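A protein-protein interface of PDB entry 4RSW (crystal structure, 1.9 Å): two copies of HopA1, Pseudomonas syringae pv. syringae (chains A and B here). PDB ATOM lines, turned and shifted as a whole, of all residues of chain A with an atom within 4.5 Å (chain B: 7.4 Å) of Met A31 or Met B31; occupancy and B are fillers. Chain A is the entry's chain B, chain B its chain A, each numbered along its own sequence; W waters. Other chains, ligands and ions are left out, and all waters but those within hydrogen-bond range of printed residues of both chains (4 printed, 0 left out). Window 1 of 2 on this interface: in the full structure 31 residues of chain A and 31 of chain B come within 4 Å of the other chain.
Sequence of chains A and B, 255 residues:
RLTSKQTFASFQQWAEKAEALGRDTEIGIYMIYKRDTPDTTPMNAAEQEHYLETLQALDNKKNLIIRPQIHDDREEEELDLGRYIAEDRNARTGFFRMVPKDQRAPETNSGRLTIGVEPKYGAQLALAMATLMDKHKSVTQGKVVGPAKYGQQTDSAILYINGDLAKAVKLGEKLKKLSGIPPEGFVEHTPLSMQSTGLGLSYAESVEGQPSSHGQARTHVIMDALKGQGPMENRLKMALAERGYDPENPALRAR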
ATOM      1  N   ILE A  27      -3.208  11.155  29.472  1.00  0.00           N
ATOM      2  CA  ILE A  27      -3.752  12.467  29.106  1.00  0.00           C
ATOM      3  C   ILE A  27      -3.047  13.611  29.832  1.00  0.00           C
ATOM      4  O   ILE A  27      -2.739  14.644  29.229  1.00  0.00           O
ATOM      5  CB  ILE A  27      -5.264  12.499  29.384  1.00  0.00           C
ATOM      6  CG1 ILE A  27      -5.956  11.544  28.415  1.00  0.00           C
ATOM      7  CG2 ILE A  27      -5.827  13.936  29.277  1.00  0.00           C
ATOM      8  CD1 ILE A  27      -7.397  11.181  28.783  1.00  0.00           C
ATOM      9  N   GLY A  28      -2.801  13.430  31.124  1.00  0.00           N
ATOM     10  CA  GLY A  28      -2.110  14.423  31.926  1.00  0.00           C
ATOM     11  C   GLY A  28      -0.679  14.640  31.466  1.00  0.00           C
ATOM     12  O   GLY A  28      -0.197  15.781  31.406  1.00  0.00           O
ATOM     13  N   ILE A  29       0.023  13.564  31.136  1.00  0.00           N
ATOM     14  CA  ILE A  29       1.361  13.759  30.581  1.00  0.00           C
ATOM     15  C   ILE A  29       1.306  14.393  29.171  1.00  0.00           C
ATOM     16  O   ILE A  29       2.059  15.320  28.868  1.00  0.00           O
ATOM     17  CB  ILE A  29       2.170  12.453  30.567  1.00  0.00           C
ATOM     18  CG1 ILE A  29       2.454  11.990  31.998  1.00  0.00           C
ATOM     19  CG2 ILE A  29       3.497  12.656  29.857  1.00  0.00           C
ATOM     20  CD1 ILE A  29       2.636  10.497  32.083  1.00  0.00           C
ATOM     21  N   TYR A  30       0.421  13.885  28.323  1.00  0.00           N
ATOM     22  CA  TYR A  30       0.236  14.413  26.963  1.00  0.00           C
ATOM     23  C   TYR A  30      -0.041  15.911  26.915  1.00  0.00           C
ATOM     24  O   TYR A  30       0.486  16.612  26.037  1.00  0.00           O
ATOM     25  CB  TYR A  30      -0.896  13.651  26.244  1.00  0.00           C
ATOM     26  CG  TYR A  30      -1.173  14.126  24.829  1.00  0.00           C
ATOM     27  CD1 TYR A  30      -0.473  13.600  23.743  1.00  0.00           C
ATOM     28  CD2 TYR A  30      -2.151  15.093  24.573  1.00  0.00           C
ATOM     29  CE1 TYR A  30      -0.736  14.033  22.439  1.00  0.00           C
ATOM     30  CE2 TYR A  30      -2.412  15.533  23.268  1.00  0.00           C
ATOM     31  CZ  TYR A  30      -1.712  14.999  22.218  1.00  0.00           C
ATOM     32  OH  TYR A  30      -1.972  15.442  20.934  1.00  0.00           O
ATOM     33  N   MET A  31      -0.857  16.409  27.845  1.00  0.00           N
ATOM     34  CA  MET A  31      -1.257  17.829  27.825  1.00  0.00           C
ATOM     35  C   MET A  31      -0.092  18.788  28.045  1.00  0.00           C
ATOM     36  O   MET A  31      -0.116  19.906  27.538  1.00  0.00           O
ATOM     37  CB  MET A  31      -2.392  18.119  28.835  1.00  0.00           C
ATOM     38  CG  MET A  31      -3.710  17.510  28.435  1.00  0.00           C
ATOM     39  SD  MET A  31      -4.276  18.153  26.687  1.00  0.00           S
ATOM     40  CE  MET A  31      -5.474  16.704  26.358  1.00  0.00           C
ATOM     41  N   ILE A  32       0.928  18.355  28.789  1.00  0.00           N
ATOM     42  CA  ILE A  32       2.119  19.174  28.987  1.00  0.00           C
ATOM     43  C   ILE A  32       2.796  19.410  27.639  1.00  0.00           C
ATOM     44  O   ILE A  32       3.205  20.532  27.333  1.00  0.00           O
ATOM     45  CB  ILE A  32       3.108  18.522  29.975  1.00  0.00           C
ATOM     46  CG1 ILE A  32       2.406  18.273  31.315  1.00  0.00           C
ATOM     47  CG2 ILE A  32       4.324  19.399  30.172  1.00  0.00           C
ATOM     48  CD1 ILE A  32       3.187  17.346  32.261  1.00  0.00           C
ATOM     49  N   TYR A  33       2.918  18.353  26.842  1.00  0.00           N
ATOM     50  CA  TYR A  33       3.406  18.480  25.474  1.00  0.00           C
ATOM     51  C   TYR A  33       2.462  19.308  24.595  1.00  0.00           C
ATOM     52  O   TYR A  33       2.905  20.194  23.848  1.00  0.00           O
ATOM     53  CB  TYR A  33       3.636  17.072  24.889  1.00  0.00           C
ATOM     54  CG  TYR A  33       3.552  16.974  23.372  1.00  0.00           C
ATOM     55  CD1 TYR A  33       4.674  17.185  22.570  1.00  0.00           C
ATOM     56  CD2 TYR A  33       2.357  16.650  22.752  1.00  0.00           C
ATOM     57  CE1 TYR A  33       4.594  17.100  21.187  1.00  0.00           C
ATOM     58  CE2 TYR A  33       2.263  16.563  21.382  1.00  0.00           C
ATOM     59  CZ  TYR A  33       3.386  16.777  20.609  1.00  0.00           C
ATOM     60  OH  TYR A  33       3.259  16.681  19.256  1.00  0.00           O
ATOM     61  N   LYS A  34       1.166  19.027  24.677  1.00  0.00           N
ATOM     62  CA  LYS A  34       0.207  19.594  23.720  1.00  0.00           C
ATOM     63  C   LYS A  34      -0.057  21.082  23.966  1.00  0.00           C
ATOM     64  O   LYS A  34      -0.146  21.860  23.004  1.00  0.00           O
ATOM     65  CB  LYS A  34      -1.116  18.807  23.739  1.00  0.00           C
ATOM     66  CG  LYS A  34      -2.067  19.091  22.568  1.00  0.00           C
ATOM     67  CD  LYS A  34      -1.413  18.792  21.197  1.00  0.00           C
ATOM     68  CE  LYS A  34      -2.476  18.672  20.114  1.00  0.00           C
ATOM     69  NZ  LYS A  34      -1.887  18.267  18.812  1.00  0.00           N
ATOM     70  N   ARG A  35      -0.158  21.473  25.239  1.00  0.00           N
ATOM     71  CA  ARG A  35      -0.564  22.848  25.589  1.00  0.00           C
ATOM     72  C   ARG A  35       0.597  23.838  25.672  1.00  0.00           C
ATOM     73  O   ARG A  35       0.436  24.990  26.077  1.00  0.00           O
ATOM     74  CB  ARG A  35      -1.372  22.855  26.890  1.00  0.00           C
ATOM     75  CG  ARG A  35      -2.734  22.170  26.726  1.00  0.00           C
ATOM     76  CD  ARG A  35      -3.447  22.106  28.058  1.00  0.00           C
ATOM     77  NE  ARG A  35      -4.789  21.561  27.914  1.00  0.00           N
ATOM     78  CZ  ARG A  35      -5.650  21.405  28.916  1.00  0.00           C
ATOM     79  NH1 ARG A  35      -5.307  21.730  30.148  1.00  0.00           N
ATOM     80  NH2 ARG A  35      -6.846  20.900  28.677  1.00  0.00           N
ATOM     81  N   HIS A 214      -2.695  11.636  17.341  1.00  0.00           N
ATOM     82  CA  HIS A 214      -2.521  12.920  18.042  1.00  0.00           C
ATOM     83  C   HIS A 214      -1.070  13.215  18.449  1.00  0.00           C
ATOM     84  O   HIS A 214      -0.823  14.139  19.229  1.00  0.00           O
ATOM     85  CB  HIS A 214      -3.461  13.043  19.263  1.00  0.00           C
ATOM     86  CG  HIS A 214      -4.905  12.825  18.933  1.00  0.00           C
ATOM     87  ND1 HIS A 214      -5.592  13.619  18.042  1.00  0.00           N
ATOM     88  CD2 HIS A 214      -5.785  11.883  19.352  1.00  0.00           C
ATOM     89  CE1 HIS A 214      -6.836  13.182  17.933  1.00  0.00           C
ATOM     90  NE2 HIS A 214      -6.978  12.132  18.717  1.00  0.00           N
ATOM     91  N   TRP B  14     -20.803   9.365  22.061  1.00  0.00           N
ATOM     92  CA  TRP B  14     -19.364   9.518  22.219  1.00  0.00           C
ATOM     93  C   TRP B  14     -18.665   8.183  22.029  1.00  0.00           C
ATOM     94  O   TRP B  14     -17.745   8.079  21.223  1.00  0.00           O
ATOM     95  CB  TRP B  14     -19.083  10.111  23.603  1.00  0.00           C
ATOM     96  CG  TRP B  14     -17.631  10.230  24.029  1.00  0.00           C
ATOM     97  CD1 TRP B  14     -16.501  10.034  23.267  1.00  0.00           C
ATOM     98  CD2 TRP B  14     -17.175  10.565  25.343  1.00  0.00           C
ATOM     99  NE1 TRP B  14     -15.373  10.222  24.046  1.00  0.00           N
ATOM    100  CE2 TRP B  14     -15.765  10.550  25.320  1.00  0.00           C
ATOM    101  CE3 TRP B  14     -17.828  10.870  26.543  1.00  0.00           C
ATOM    102  CZ2 TRP B  14     -14.998  10.830  26.458  1.00  0.00           C
ATOM    103  CZ3 TRP B  14     -17.065  11.150  27.671  1.00  0.00           C
ATOM    104  CH2 TRP B  14     -15.666  11.128  27.620  1.00  0.00           C
ATOM    105  N   ARG B  23     -10.801   5.053  17.061  1.00  0.00           N
ATOM    106  CA  ARG B  23      -9.988   5.468  18.208  1.00  0.00           C
ATOM    107  C   ARG B  23      -9.947   4.369  19.269  1.00  0.00           C
ATOM    108  O   ARG B  23     -10.980   3.831  19.655  1.00  0.00           O
ATOM    109  CB  ARG B  23     -10.500   6.773  18.835  1.00  0.00           C
ATOM    110  CG  ARG B  23     -10.789   7.891  17.846  1.00  0.00           C
ATOM    111  CD  ARG B  23      -9.531   8.374  17.100  1.00  0.00           C
ATOM    112  NE  ARG B  23      -9.806   9.629  16.404  1.00  0.00           N
ATOM    113  CZ  ARG B  23      -9.898   9.763  15.082  1.00  0.00           C
ATOM    114  NH1 ARG B  23      -9.695   8.718  14.278  1.00  0.00           N
ATOM    115  NH2 ARG B  23     -10.182  10.952  14.562  1.00  0.00           N
ATOM    116  N   THR B  25      -7.258   4.632  21.970  1.00  0.00           N
ATOM    117  CA  THR B  25      -6.393   5.075  23.073  1.00  0.00           C
ATOM    118  C   THR B  25      -7.127   6.062  23.981  1.00  0.00           C
ATOM    119  O   THR B  25      -8.132   6.653  23.584  1.00  0.00           O
ATOM    120  CB  THR B  25      -5.086   5.723  22.562  1.00  0.00           C
ATOM    121  OG1 THR B  25      -5.390   6.928  21.846  1.00  0.00           O
ATOM    122  CG2 THR B  25      -4.340   4.763  21.632  1.00  0.00           C
ATOM    123  N   GLU B  26      -6.619   6.248  25.193  1.00  0.00           N
ATOM    124  CA  GLU B  26      -7.236   7.185  26.126  1.00  0.00           C
ATOM    125  C   GLU B  26      -7.258   8.585  25.545  1.00  0.00           C
ATOM    126  O   GLU B  26      -8.281   9.278  25.594  1.00  0.00           O
ATOM    127  CB  GLU B  26      -6.503   7.166  27.464  1.00  0.00           C
ATOM    128  CG  GLU B  26      -6.905   5.964  28.334  1.00  0.00           C
ATOM    129  CD  GLU B  26      -5.993   5.749  29.518  1.00  0.00           C
ATOM    130  OE1 GLU B  26      -5.401   6.743  30.029  1.00  0.00           O
ATOM    131  OE2 GLU B  26      -5.863   4.571  29.932  1.00  0.00           O
ATOM    132  N   ILE B  27      -6.136   8.997  24.965  1.00  0.00           N
ATOM    133  CA  ILE B  27      -6.064  10.339  24.387  1.00  0.00           C
ATOM    134  C   ILE B  27      -7.036  10.498  23.229  1.00  0.00           C
ATOM    135  O   ILE B  27      -7.715  11.512  23.150  1.00  0.00           O
ATOM    136  CB  ILE B  27      -4.633  10.697  23.950  1.00  0.00           C
ATOM    137  CG1 ILE B  27      -3.756  10.891  25.189  1.00  0.00           C
ATOM    138  CG2 ILE B  27      -4.611  11.983  23.121  1.00  0.00           C
ATOM    139  CD1 ILE B  27      -2.260  10.640  24.917  1.00  0.00           C
ATOM    140  N   GLY B  28      -7.111   9.491  22.353  1.00  0.00           N
ATOM    141  CA  GLY B  28      -7.967   9.548  21.178  1.00  0.00           C
ATOM    142  C   GLY B  28      -9.446   9.604  21.524  1.00  0.00           C
ATOM    143  O   GLY B  28     -10.220  10.343  20.899  1.00  0.00           O
ATOM    144  N   ILE B  29      -9.848   8.820  22.518  1.00  0.00           N
ATOM    145  CA  ILE B  29     -11.227   8.862  23.002  1.00  0.00           C
ATOM    146  C   ILE B  29     -11.516  10.223  23.639  1.00  0.00           C
ATOM    147  O   ILE B  29     -12.543  10.845  23.370  1.00  0.00           O
ATOM    148  CB  ILE B  29     -11.469   7.776  24.065  1.00  0.00           C
ATOM    149  CG1 ILE B  29     -11.459   6.377  23.435  1.00  0.00           C
ATOM    150  CG2 ILE B  29     -12.808   7.986  24.759  1.00  0.00           C
ATOM    151  CD1 ILE B  29     -11.186   5.283  24.472  1.00  0.00           C
ATOM    152  N   TYR B  30     -10.616  10.668  24.505  1.00  0.00           N
ATOM    153  CA  TYR B  30     -10.803  11.933  25.228  1.00  0.00           C
ATOM    154  C   TYR B  30     -10.972  13.124  24.294  1.00  0.00           C
ATOM    155  O   TYR B  30     -11.752  14.023  24.581  1.00  0.00           O
ATOM    156  CB  TYR B  30      -9.613  12.179  26.158  1.00  0.00           C
ATOM    157  CG  TYR B  30      -9.622  13.508  26.900  1.00  0.00           C
ATOM    158  CD1 TYR B  30     -10.323  13.653  28.083  1.00  0.00           C
ATOM    159  CD2 TYR B  30      -8.890  14.608  26.432  1.00  0.00           C
ATOM    160  CE1 TYR B  30     -10.328  14.847  28.767  1.00  0.00           C
ATOM    161  CE2 TYR B  30      -8.889  15.815  27.122  1.00  0.00           C
ATOM    162  CZ  TYR B  30      -9.614  15.923  28.286  1.00  0.00           C
ATOM    163  OH  TYR B  30      -9.634  17.112  28.995  1.00  0.00           O
ATOM    164  N   MET B  31     -10.233  13.146  23.182  1.00  0.00           N
ATOM    165  CA  MET B  31     -10.289  14.302  22.285  1.00  0.00           C
ATOM    166  C   MET B  31     -11.652  14.478  21.631  1.00  0.00           C
ATOM    167  O   MET B  31     -12.046  15.598  21.299  1.00  0.00           O
ATOM    168  CB  MET B  31      -9.188  14.233  21.214  1.00  0.00           C
ATOM    169  CG  MET B  31      -7.795  14.428  21.777  1.00  0.00           C
ATOM    170  SD  MET B  31      -7.593  16.140  22.730  1.00  0.00           S
ATOM    171  CE  MET B  31      -5.659  16.183  22.721  1.00  0.00           C
ATOM    172  N   ILE B  32     -12.391  13.388  21.459  1.00  0.00           N
ATOM    173  CA  ILE B  32     -13.738  13.495  20.914  1.00  0.00           C
ATOM    174  C   ILE B  32     -14.606  14.319  21.871  1.00  0.00           C
ATOM    175  O   ILE B  32     -15.388  15.167  21.448  1.00  0.00           O
ATOM    176  CB  ILE B  32     -14.355  12.093  20.709  1.00  0.00           C
ATOM    177  CG1 ILE B  32     -13.515  11.287  19.715  1.00  0.00           C
ATOM    178  CG2 ILE B  32     -15.784  12.183  20.204  1.00  0.00           C
ATOM    179  CD1 ILE B  32     -13.860   9.820  19.696  1.00  0.00           C
ATOM    180  N   TYR B  33     -14.471  14.051  23.160  1.00  0.00           N
ATOM    181  CA  TYR B  33     -15.156  14.811  24.193  1.00  0.00           C
ATOM    182  C   TYR B  33     -14.636  16.242  24.258  1.00  0.00           C
ATOM    183  O   TYR B  33     -15.410  17.196  24.307  1.00  0.00           O
ATOM    184  CB  TYR B  33     -14.951  14.096  25.529  1.00  0.00           C
ATOM    185  CG  TYR B  33     -15.043  14.961  26.768  1.00  0.00           C
ATOM    186  CD1 TYR B  33     -16.269  15.263  27.344  1.00  0.00           C
ATOM    187  CD2 TYR B  33     -13.894  15.450  27.374  1.00  0.00           C
ATOM    188  CE1 TYR B  33     -16.345  16.044  28.476  1.00  0.00           C
ATOM    189  CE2 TYR B  33     -13.955  16.226  28.498  1.00  0.00           C
ATOM    190  CZ  TYR B  33     -15.183  16.520  29.038  1.00  0.00           C
ATOM    191  OH  TYR B  33     -15.241  17.286  30.159  1.00  0.00           O
ATOM    192  N   LYS B  34     -13.320  16.392  24.240  1.00  0.00           N
ATOM    193  CA  LYS B  34     -12.705  17.703  24.486  1.00  0.00           C
ATOM    194  C   LYS B  34     -12.892  18.690  23.327  1.00  0.00           C
ATOM    195  O   LYS B  34     -13.183  19.872  23.557  1.00  0.00           O
ATOM    196  CB  LYS B  34     -11.221  17.523  24.847  1.00  0.00           C
ATOM    197  CG  LYS B  34     -10.525  18.775  25.431  1.00  0.00           C
ATOM    198  CD  LYS B  34     -11.218  19.277  26.706  1.00  0.00           C
ATOM    199  CE  LYS B  34     -10.269  20.087  27.578  1.00  0.00           C
ATOM    200  NZ  LYS B  34     -10.873  20.362  28.919  1.00  0.00           N
ATOM    201  N   ARG B  35     -12.760  18.216  22.084  1.00  0.00           N
ATOM    202  CA  ARG B  35     -12.759  19.133  20.937  1.00  0.00           C
ATOM    203  C   ARG B  35     -14.152  19.408  20.364  1.00  0.00           C
ATOM    204  O   ARG B  35     -14.318  20.036  19.302  1.00  0.00           O
ATOM    205  CB  ARG B  35     -11.830  18.610  19.840  1.00  0.00           C
ATOM    206  CG  ARG B  35     -10.387  18.565  20.253  1.00  0.00           C
ATOM    207  CD  ARG B  35      -9.494  18.044  19.118  1.00  0.00           C
ATOM    208  NE  ARG B  35      -8.116  17.961  19.575  1.00  0.00           N
ATOM    209  CZ  ARG B  35      -7.115  17.430  18.887  1.00  0.00           C
ATOM    210  NH1 ARG B  35      -7.337  16.909  17.698  1.00  0.00           N
ATOM    211  NH2 ARG B  35      -5.888  17.408  19.400  1.00  0.00           N
ATOM    212  N   ASP B  36     -15.151  18.929  21.080  1.00  0.00           N
ATOM    213  CA  ASP B  36     -16.548  19.158  20.759  1.00  0.00           C
ATOM    214  C   ASP B  36     -16.848  20.646  20.996  1.00  0.00           C
ATOM    215  O   ASP B  36     -17.027  21.078  22.136  1.00  0.00           O
ATOM    216  CB  ASP B  36     -17.335  18.247  21.695  1.00  0.00           C
ATOM    217  CG  ASP B  36     -18.830  18.443  21.621  1.00  0.00           C
ATOM    218  OD1 ASP B  36     -19.364  18.796  20.543  1.00  0.00           O
ATOM    219  OD2 ASP B  36     -19.466  18.197  22.669  1.00  0.00           O
ATOM    220  N   GLN B  69      -2.445  25.990  35.890  1.00  0.00           N
ATOM    221  CA  GLN B  69      -2.273  24.581  36.200  1.00  0.00           C
ATOM    222  C   GLN B  69      -0.848  24.138  35.971  1.00  0.00           C
ATOM    223  O   GLN B  69      -0.353  23.262  36.681  1.00  0.00           O
ATOM    224  CB  GLN B  69      -3.218  23.704  35.383  1.00  0.00           C
ATOM    225  CG  GLN B  69      -4.644  23.817  35.829  1.00  0.00           C
ATOM    226  CD  GLN B  69      -5.553  22.832  35.143  1.00  0.00           C
ATOM    227  OE1 GLN B  69      -6.540  22.404  35.726  1.00  0.00           O
ATOM    228  NE2 GLN B  69      -5.247  22.488  33.887  1.00  0.00           N
ATOM    229  N   ILE B  70      -0.176  24.782  35.022  1.00  0.00           N
ATOM    230  CA  ILE B  70       1.205  24.440  34.686  1.00  0.00           C
ATOM    231  C   ILE B  70       2.154  24.836  35.833  1.00  0.00           C
ATOM    232  O   ILE B  70       3.353  24.542  35.792  1.00  0.00           O
ATOM    233  CB  ILE B  70       1.633  25.123  33.362  1.00  0.00           C
ATOM    234  CG1 ILE B  70       2.873  24.445  32.772  1.00  0.00           C
ATOM    235  CG2 ILE B  70       1.879  26.602  33.579  1.00  0.00           C
ATOM    236  CD1 ILE B  70       2.644  23.000  32.376  1.00  0.00           C
ATOM    237  N   LEU B 192     -20.090  15.983  26.450  1.00  0.00           N
ATOM    238  CA  LEU B 192     -20.563  14.604  26.340  1.00  0.00           C
ATOM    239  C   LEU B 192     -20.511  13.879  27.693  1.00  0.00           C
ATOM    240  O   LEU B 192     -19.536  14.024  28.429  1.00  0.00           O
ATOM    241  CB  LEU B 192     -19.766  13.853  25.278  1.00  0.00           C
ATOM    242  CG  LEU B 192     -19.760  14.591  23.924  1.00  0.00           C
ATOM    243  CD1 LEU B 192     -18.880  13.890  22.915  1.00  0.00           C
ATOM    244  CD2 LEU B 192     -21.178  14.750  23.383  1.00  0.00           C
ATOM    245  N   HIS B 214      -8.100  16.933  34.106  1.00  0.00           N
ATOM    246  CA  HIS B 214      -8.608  17.364  32.802  1.00  0.00           C
ATOM    247  C   HIS B 214     -10.011  16.845  32.480  1.00  0.00           C
ATOM    248  O   HIS B 214     -10.451  16.923  31.344  1.00  0.00           O
ATOM    249  CB  HIS B 214      -7.627  16.986  31.680  1.00  0.00           C
ATOM    250  CG  HIS B 214      -6.230  17.468  31.912  1.00  0.00           C
ATOM    251  ND1 HIS B 214      -5.884  18.805  31.871  1.00  0.00           N
ATOM    252  CD2 HIS B 214      -5.087  16.794  32.196  1.00  0.00           C
ATOM    253  CE1 HIS B 214      -4.591  18.930  32.111  1.00  0.00           C
ATOM    254  NE2 HIS B 214      -4.083  17.725  32.310  1.00  0.00           N
ATOM    255  N   THR B 219     -13.660   8.809  30.033  1.00  0.00           N
ATOM    256  CA  THR B 219     -12.814   8.209  29.001  1.00  0.00           C
ATOM    257  C   THR B 219     -12.433   6.762  29.331  1.00  0.00           C
ATOM    258  O   THR B 219     -12.412   5.890  28.457  1.00  0.00           O
ATOM    259  CB  THR B 219     -11.525   9.059  28.786  1.00  0.00           C
ATOM    260  OG1 THR B 219     -11.883  10.305  28.160  1.00  0.00           O
ATOM    261  CG2 THR B 219     -10.516   8.314  27.898  1.00  0.00           C
HETATM  262  O   HOH W   1      -5.149   9.200  30.630  1.00  0.00           O
HETATM  263  O   HOH W   2      -1.333  18.094  32.575  1.00  0.00           O
HETATM  264  O   HOH W   3      -9.714  11.559  18.499  1.00  0.00           O
HETATM  265  O   HOH W   4      -4.105  16.417  17.080  1.00  0.00           O
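The side-chain hydroxyl (OG1) of Thr B25 is in hydrogen-bond range of the backbone NH (N) of Gly B28 (3.1 Å).
The side-chain hydroxyl (OH) of Tyr B30 lies close to the side-chain amino group (NZ) of Lys B34, 3.5 Å away.
OH of Tyr B30 sits at hydrogen-bond distance from O of His B214 (2.5 Å).
NE of Arg B35 sits at hydrogen-bond distance from SD of Met B31 (3.7 Å).
O of His A214 sits at hydrogen-bond distance from OH of Tyr A30 (2.4 Å).
The guanidinium group (NE) of Arg A35 lies within hydrogen-bond range of the side-chain sulfur (SD) of Met A31 (3.7 Å).
Tyr A30 touches Met B31, and with the chains exchanged Met A31 touches Tyr B30.
Met A31 touches His B214, and with the chains exchanged His A214 touches Met B31.
Arg A35 touches His B214, and with the chains exchanged His A214 touches Arg B35.
His A214 touches Ile B27, but with the chains exchanged Ile A27 does not touch His B214 (4.2 Å).
Positions printed for both chains: 27, 28, 29, 30, 31, 32, 33, 34, 35 and 214.
Of the 17 pairs that touch across the chains among the printed residues, 14 have their exchanged pair printed and touching as well.
CG1 of Ile A27 touches CG1 of Ile B27 (3.96 Å).
Ile B27 touches Tyr A30.
CE of Met A31 touches CE2 of Tyr B30, 3.6 Å away.
Met A31 touches Met B31.
His B214 touches Met A31.
CE of Lys A34 touches NH2 of Arg B35, at 3.7 Å.
Arg A35 touches Lys B34.
His A214 touches Ile B27 (CD2 to CG2, 3.9 Å).
His A214 touches Gly B28.
ND1 of His A214 touches NH1 of Arg B35 (3.7 Å).
Of chain B, only Tyr B30, Met B31 and His B214 come within 4 Å of Met A31.
Of the printed residues of chain A, Gly B28 touches His A214 (3.7 Å).
Of the printed residues of chain A, Arg B35 touches Lys A34 (3.7 Å) and His A214 (3.7 Å).
Printed residues of chain B within 4 Å of Gly A28: His B214 (3.8 Å).
Of the printed residues of chain A, Lys B34 touches Arg A35 (3.7 Å).
Ile A32 touches none of the printed residues of chain B.
The nearest printed residue of chain A that does not touch Met B31 is Lys A34 (4.6 Å).
The nearest printed residue of chain B that does not touch Ile A27 is His B214 (4.2 Å).
Water W1 bridges the side-chain carboxylate (OE1) of Glu B26 and the backbone NH (N) of Ile A27.
Water W3 lies within hydrogen-bond range of the backbone carbonyl oxygen (O) of Gly B28 (2.7 Å), a ring nitrogen (NE2) of His A214 (2.8 Å) and the guanidinium group (NE) of Arg B23 (2.8 Å).
Water W2 bridges a ring nitrogen (NE2) of His B214 and the backbone carbonyl oxygen of Gly A28.
Water W4 lies within hydrogen-bond range of the guanidinium group of Arg B35, a ring nitrogen (ND1) of His A214 and the side-chain amino group of Lys A34.
Of the 10 printed residues of chain A, 7 touch a printed residue of chain B.
Of the 19 printed residues of chain B, 9 touch a printed residue of chain A.
Among the printed residues, no Asp or Glu carboxylate lies within 4 Å of a Lys or Arg side-chain nitrogen of the other chain.
A ring nitrogen (ND1) of His B214 lies within hydrogen-bond range of the guanidinium group (NH1) of Arg A35 (3.4 Å).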
